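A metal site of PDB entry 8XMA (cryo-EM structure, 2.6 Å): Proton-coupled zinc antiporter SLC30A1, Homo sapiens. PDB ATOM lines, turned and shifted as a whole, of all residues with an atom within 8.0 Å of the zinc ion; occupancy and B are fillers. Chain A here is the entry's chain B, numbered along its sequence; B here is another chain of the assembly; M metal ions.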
ATOM      1  N   GLU A 368     -23.721  19.434  -4.157  1.00  0.00           N
ATOM      2  CA  GLU A 368     -24.856  20.058  -4.815  1.00  0.00           C
ATOM      3  C   GLU A 368     -24.701  19.876  -6.318  1.00  0.00           C
ATOM      4  O   GLU A 368     -23.592  19.796  -6.837  1.00  0.00           O
ATOM      5  CB  GLU A 368     -24.979  21.545  -4.444  1.00  0.00           C
ATOM      6  CG  GLU A 368     -23.802  22.419  -4.848  1.00  0.00           C
ATOM      7  CD  GLU A 368     -23.902  22.932  -6.276  1.00  0.00           C
ATOM      8  OE1 GLU A 368     -25.026  22.931  -6.820  1.00  0.00           O
ATOM      9  OE2 GLU A 368     -22.867  23.320  -6.837  1.00  0.00           O
ATOM     10  N   VAL A 369     -25.844  19.810  -7.011  1.00  0.00           N
ATOM     11  CA  VAL A 369     -25.880  19.607  -8.447  1.00  0.00           C
ATOM     12  C   VAL A 369     -26.578  20.796  -9.094  1.00  0.00           C
ATOM     13  O   VAL A 369     -27.701  21.129  -8.727  1.00  0.00           O
ATOM     14  CB  VAL A 369     -26.599  18.293  -8.814  1.00  0.00           C
ATOM     15  CG1 VAL A 369     -26.722  18.168 -10.328  1.00  0.00           C
ATOM     16  CG2 VAL A 369     -25.859  17.097  -8.227  1.00  0.00           C
ATOM     17  N   HIS A 370     -25.896  21.427 -10.051  1.00  0.00           N
ATOM     18  CA  HIS A 370     -26.459  22.565 -10.769  1.00  0.00           C
ATOM     19  C   HIS A 370     -26.125  22.443 -12.243  1.00  0.00           C
ATOM     20  O   HIS A 370     -25.230  21.689 -12.639  1.00  0.00           O
ATOM     21  CB  HIS A 370     -25.929  23.897 -10.206  1.00  0.00           C
ATOM     22  CG  HIS A 370     -24.490  24.138 -10.503  1.00  0.00           C
ATOM     23  ND1 HIS A 370     -23.475  23.573  -9.772  1.00  0.00           N
ATOM     24  CD2 HIS A 370     -23.891  24.914 -11.443  1.00  0.00           C
ATOM     25  CE1 HIS A 370     -22.308  23.969 -10.253  1.00  0.00           C
ATOM     26  NE2 HIS A 370     -22.532  24.784 -11.271  1.00  0.00           N
ATOM     27  N   GLU A 371     -26.872  23.175 -13.062  1.00  0.00           N
ATOM     28  CA  GLU A 371     -26.738  23.153 -14.516  1.00  0.00           C
ATOM     29  C   GLU A 371     -26.946  21.736 -15.060  1.00  0.00           C
ATOM     30  O   GLU A 371     -26.100  21.170 -15.744  1.00  0.00           O
ATOM     31  CB  GLU A 371     -25.380  23.725 -14.941  1.00  0.00           C
ATOM     32  CG  GLU A 371     -25.297  24.113 -16.408  1.00  0.00           C
ATOM     33  CD  GLU A 371     -25.986  25.427 -16.698  1.00  0.00           C
ATOM     34  OE1 GLU A 371     -26.013  26.302 -15.807  1.00  0.00           O
ATOM     35  OE2 GLU A 371     -26.507  25.589 -17.823  1.00  0.00           O
ATOM     36  N   LEU A 372     -28.099  21.176 -14.716  1.00  0.00           N
ATOM     37  CA  LEU A 372     -28.485  19.848 -15.197  1.00  0.00           C
ATOM     38  C   LEU A 372     -29.289  19.998 -16.480  1.00  0.00           C
ATOM     39  O   LEU A 372     -30.358  20.608 -16.484  1.00  0.00           O
ATOM     40  CB  LEU A 372     -29.313  19.101 -14.143  1.00  0.00           C
ATOM     41  CG  LEU A 372     -29.790  17.721 -14.592  1.00  0.00           C
ATOM     42  CD1 LEU A 372     -28.692  16.693 -14.442  1.00  0.00           C
ATOM     43  CD2 LEU A 372     -31.031  17.301 -13.822  1.00  0.00           C
ATOM     44  N   ALA A 386     -24.328  17.741 -16.368  1.00  0.00           N
ATOM     45  CA  ALA A 386     -24.497  18.355 -15.056  1.00  0.00           C
ATOM     46  C   ALA A 386     -23.157  18.815 -14.514  1.00  0.00           C
ATOM     47  O   ALA A 386     -22.093  18.333 -14.916  1.00  0.00           O
ATOM     48  CB  ALA A 386     -25.156  17.378 -14.073  1.00  0.00           C
ATOM     49  N   HIS A 387     -23.218  19.761 -13.587  1.00  0.00           N
ATOM     50  CA  HIS A 387     -22.061  20.237 -12.842  1.00  0.00           C
ATOM     51  C   HIS A 387     -22.226  19.832 -11.380  1.00  0.00           C
ATOM     52  O   HIS A 387     -23.326  19.946 -10.819  1.00  0.00           O
ATOM     53  CB  HIS A 387     -21.910  21.758 -12.945  1.00  0.00           C
ATOM     54  CG  HIS A 387     -21.685  22.255 -14.336  1.00  0.00           C
ATOM     55  ND1 HIS A 387     -21.291  23.549 -14.607  1.00  0.00           N
ATOM     56  CD2 HIS A 387     -21.814  21.639 -15.539  1.00  0.00           C
ATOM     57  CE1 HIS A 387     -21.184  23.701 -15.911  1.00  0.00           C
ATOM     58  NE2 HIS A 387     -21.499  22.565 -16.499  1.00  0.00           N
ATOM     59  N   ILE A 388     -21.147  19.368 -10.764  1.00  0.00           N
ATOM     60  CA  ILE A 388     -21.200  18.897  -9.384  1.00  0.00           C
ATOM     61  C   ILE A 388     -20.069  19.534  -8.597  1.00  0.00           C
ATOM     62  O   ILE A 388     -19.059  19.979  -9.161  1.00  0.00           O
ATOM     63  CB  ILE A 388     -21.101  17.359  -9.290  1.00  0.00           C
ATOM     64  CG1 ILE A 388     -19.832  16.868  -9.964  1.00  0.00           C
ATOM     65  CG2 ILE A 388     -22.335  16.712  -9.918  1.00  0.00           C
ATOM     66  CD1 ILE A 388     -19.511  15.418  -9.679  1.00  0.00           C
ATOM     67  N   LYS A 389     -20.234  19.593  -7.278  1.00  0.00           N
ATOM     68  CA  LYS A 389     -19.203  20.019  -6.353  1.00  0.00           C
ATOM     69  C   LYS A 389     -18.871  18.864  -5.428  1.00  0.00           C
ATOM     70  O   LYS A 389     -19.770  18.315  -4.772  1.00  0.00           O
ATOM     71  CB  LYS A 389     -19.644  21.241  -5.555  1.00  0.00           C
ATOM     72  CG  LYS A 389     -19.682  22.536  -6.360  1.00  0.00           C
ATOM     73  CD  LYS A 389     -20.015  23.717  -5.476  1.00  0.00           C
ATOM     74  CE  LYS A 389     -20.120  25.002  -6.283  1.00  0.00           C
ATOM     75  NZ  LYS A 389     -18.791  25.440  -6.803  1.00  0.00           N
ATOM     76  N   GLN A 418     -19.219  17.548 -14.965  1.00  0.00           N
ATOM     77  CA  GLN A 418     -18.055  18.404 -14.732  1.00  0.00           C
ATOM     78  C   GLN A 418     -17.932  18.710 -13.257  1.00  0.00           C
ATOM     79  O   GLN A 418     -18.793  19.413 -12.706  1.00  0.00           O
ATOM     80  CB  GLN A 418     -18.173  19.691 -15.541  1.00  0.00           C
ATOM     81  CG  GLN A 418     -17.211  20.781 -15.105  1.00  0.00           C
ATOM     82  CD  GLN A 418     -17.660  22.161 -15.530  1.00  0.00           C
ATOM     83  OE1 GLN A 418     -17.888  22.408 -16.708  1.00  0.00           O
ATOM     84  NE2 GLN A 418     -17.783  23.060 -14.567  1.00  0.00           N
ATOM     85  N   PRO A 419     -16.900  18.221 -12.571  1.00  0.00           N
ATOM     86  CA  PRO A 419     -16.734  18.539 -11.153  1.00  0.00           C
ATOM     87  C   PRO A 419     -16.245  19.969 -10.963  1.00  0.00           C
ATOM     88  O   PRO A 419     -15.618  20.567 -11.845  1.00  0.00           O
ATOM     89  CB  PRO A 419     -15.677  17.536 -10.674  1.00  0.00           C
ATOM     90  CG  PRO A 419     -15.450  16.600 -11.823  1.00  0.00           C
ATOM     91  CD  PRO A 419     -15.849  17.323 -13.055  1.00  0.00           C
ATOM     92  N   GLU A 420     -16.543  20.514  -9.791  1.00  0.00           N
ATOM     93  CA  GLU A 420     -16.027  21.810  -9.372  1.00  0.00           C
ATOM     94  C   GLU A 420     -15.556  21.697  -7.929  1.00  0.00           C
ATOM     95  O   GLU A 420     -16.255  21.118  -7.088  1.00  0.00           O
ATOM     96  CB  GLU A 420     -17.078  22.909  -9.499  1.00  0.00           C
ATOM     97  CG  GLU A 420     -17.709  23.007 -10.883  1.00  0.00           C
ATOM     98  CD  GLU A 420     -18.886  23.968 -10.923  1.00  0.00           C
ATOM     99  OE1 GLU A 420     -19.031  24.772  -9.984  1.00  0.00           O
ATOM    100  OE2 GLU A 420     -19.654  23.909 -11.901  1.00  0.00           O
ATOM    101  N   PRO A 432     -22.438  30.743  -7.762  1.00  0.00           N
ATOM    102  CA  PRO A 432     -23.184  29.516  -8.069  1.00  0.00           C
ATOM    103  C   PRO A 432     -22.357  28.495  -8.842  1.00  0.00           C
ATOM    104  O   PRO A 432     -22.495  27.290  -8.607  1.00  0.00           O
ATOM    105  CB  PRO A 432     -24.389  30.021  -8.875  1.00  0.00           C
ATOM    106  CG  PRO A 432     -23.930  31.322  -9.447  1.00  0.00           C
ATOM    107  CD  PRO A 432     -23.029  31.926  -8.418  1.00  0.00           C
ATOM    108  N   CYS A 433     -21.519  28.963  -9.762  1.00  0.00           N
ATOM    109  CA  CYS A 433     -20.701  28.074 -10.582  1.00  0.00           C
ATOM    110  C   CYS A 433     -19.298  28.646 -10.728  1.00  0.00           C
ATOM    111  O   CYS A 433     -19.129  29.727 -11.302  1.00  0.00           O
ATOM    112  CB  CYS A 433     -21.343  27.864 -11.955  1.00  0.00           C
ATOM    113  SG  CYS A 433     -20.463  26.725 -13.055  1.00  0.00           S
ATOM    114  N   GLU A 434     -18.302  27.935 -10.222  1.00  0.00           N
ATOM    115  CA  GLU A 434     -16.920  28.434 -10.280  1.00  0.00           C
ATOM    116  C   GLU A 434     -16.393  28.580 -11.700  1.00  0.00           C
ATOM    117  O   GLU A 434     -15.716  29.569 -12.010  1.00  0.00           O
ATOM    118  CB  GLU A 434     -16.002  27.514  -9.482  1.00  0.00           C
ATOM    119  CG  GLU A 434     -16.250  27.559  -7.995  1.00  0.00           C
ATOM    120  CD  GLU A 434     -15.777  26.296  -7.306  1.00  0.00           C
ATOM    121  OE1 GLU A 434     -15.375  25.353  -8.018  1.00  0.00           O
ATOM    122  OE2 GLU A 434     -15.825  26.246  -6.060  1.00  0.00           O
ATOM    123  N   LEU A 435     -16.693  27.619 -12.563  1.00  0.00           N
ATOM    124  CA  LEU A 435     -16.256  27.722 -13.949  1.00  0.00           C
ATOM    125  C   LEU A 435     -17.247  28.560 -14.739  1.00  0.00           C
ATOM    126  O   LEU A 435     -18.076  28.031 -15.475  1.00  0.00           O
ATOM    127  CB  LEU A 435     -16.125  26.338 -14.584  1.00  0.00           C
ATOM    128  CG  LEU A 435     -14.754  25.671 -14.458  1.00  0.00           C
ATOM    129  CD1 LEU A 435     -14.692  24.453 -15.359  1.00  0.00           C
ATOM    130  CD2 LEU A 435     -13.674  26.660 -14.843  1.00  0.00           C
ATOM    131  N   ALA A 436     -17.146  29.885 -14.596  1.00  0.00           N
ATOM    132  CA  ALA A 436     -18.090  30.759 -15.281  1.00  0.00           C
ATOM    133  C   ALA A 436     -17.332  31.665 -16.234  1.00  0.00           C
ATOM    134  O   ALA A 436     -16.134  31.931 -16.067  1.00  0.00           O
ATOM    135  CB  ALA A 436     -18.897  31.597 -14.287  1.00  0.00           C
ATOM    136  N   LYS B 404     -11.610  26.498 -20.107  1.00  0.00           N
ATOM    137  CA  LYS B 404     -12.688  27.488 -20.167  1.00  0.00           C
ATOM    138  C   LYS B 404     -12.257  28.714 -20.947  1.00  0.00           C
ATOM    139  O   LYS B 404     -13.017  29.260 -21.744  1.00  0.00           O
ATOM    140  CB  LYS B 404     -13.137  27.865 -18.764  1.00  0.00           C
ATOM    141  CG  LYS B 404     -14.288  28.860 -18.723  1.00  0.00           C
ATOM    142  CD  LYS B 404     -15.558  28.308 -19.335  1.00  0.00           C
ATOM    143  CE  LYS B 404     -16.146  27.215 -18.468  1.00  0.00           C
ATOM    144  NZ  LYS B 404     -17.429  26.707 -19.017  1.00  0.00           N
ATOM    145  N   THR B 415     -20.095  25.675 -21.447  1.00  0.00           N
ATOM    146  CA  THR B 415     -19.332  24.464 -21.673  1.00  0.00           C
ATOM    147  C   THR B 415     -19.503  23.491 -20.501  1.00  0.00           C
ATOM    148  O   THR B 415     -20.085  23.816 -19.467  1.00  0.00           O
ATOM    149  CB  THR B 415     -17.845  24.783 -21.867  1.00  0.00           C
ATOM    150  OG1 THR B 415     -17.249  25.089 -20.601  1.00  0.00           O
ATOM    151  CG2 THR B 415     -17.682  25.972 -22.785  1.00  0.00           C
ATOM    152  N   THR B 416     -18.986  22.285 -20.712  1.00  0.00           N
ATOM    153  CA  THR B 416     -18.966  21.263 -19.669  1.00  0.00           C
ATOM    154  C   THR B 416     -17.835  20.295 -19.989  1.00  0.00           C
ATOM    155  O   THR B 416     -17.898  19.586 -20.997  1.00  0.00           O
ATOM    156  CB  THR B 416     -20.297  20.527 -19.588  1.00  0.00           C
ATOM    157  OG1 THR B 416     -21.335  21.440 -19.215  1.00  0.00           O
ATOM    158  CG2 THR B 416     -20.221  19.414 -18.551  1.00  0.00           C
HETATM  159 ZN    ZN M   1     -21.288  24.534 -12.841  1.00  0.00          ZN
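Within 4 Å of the zinc ion: His 370, His 387, Glu 420 and Cys 433.
OE2 of Glu 420 sits close to NE2 of Gln 418, at 3.4 Å. OE1 of Glu 420 lies within hydrogen-bond range of N of Glu 434 (3.3 Å). OE1 of Glu 420 lies within salt-bridge range of NZ of Lys 389, 3.3 Å away. The backbone NH of Glu 420 is in hydrogen-bond range of the backbone carbonyl oxygen of Ile 388. ND1 of His 370 lies within hydrogen-bond range of OE2 of Glu 368 (3.0 Å). A ring nitrogen (NE2) of His 387 is in hydrogen-bond range of the side-chain hydroxyl of Thr 416 of chain B, 2.9 Å away. The backbone carbonyl oxygen (O) of Leu 435 lies close to the side-chain sulfur (SG) of Cys 433 (3.6 Å).
The zinc ion is bound by OE2 of Glu 420 (2.0 Å), NE2 of His 370 (2.0 Å), ND1 of His 387 (2.0 Å) and SG of Cys 433 (2.4 Å).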
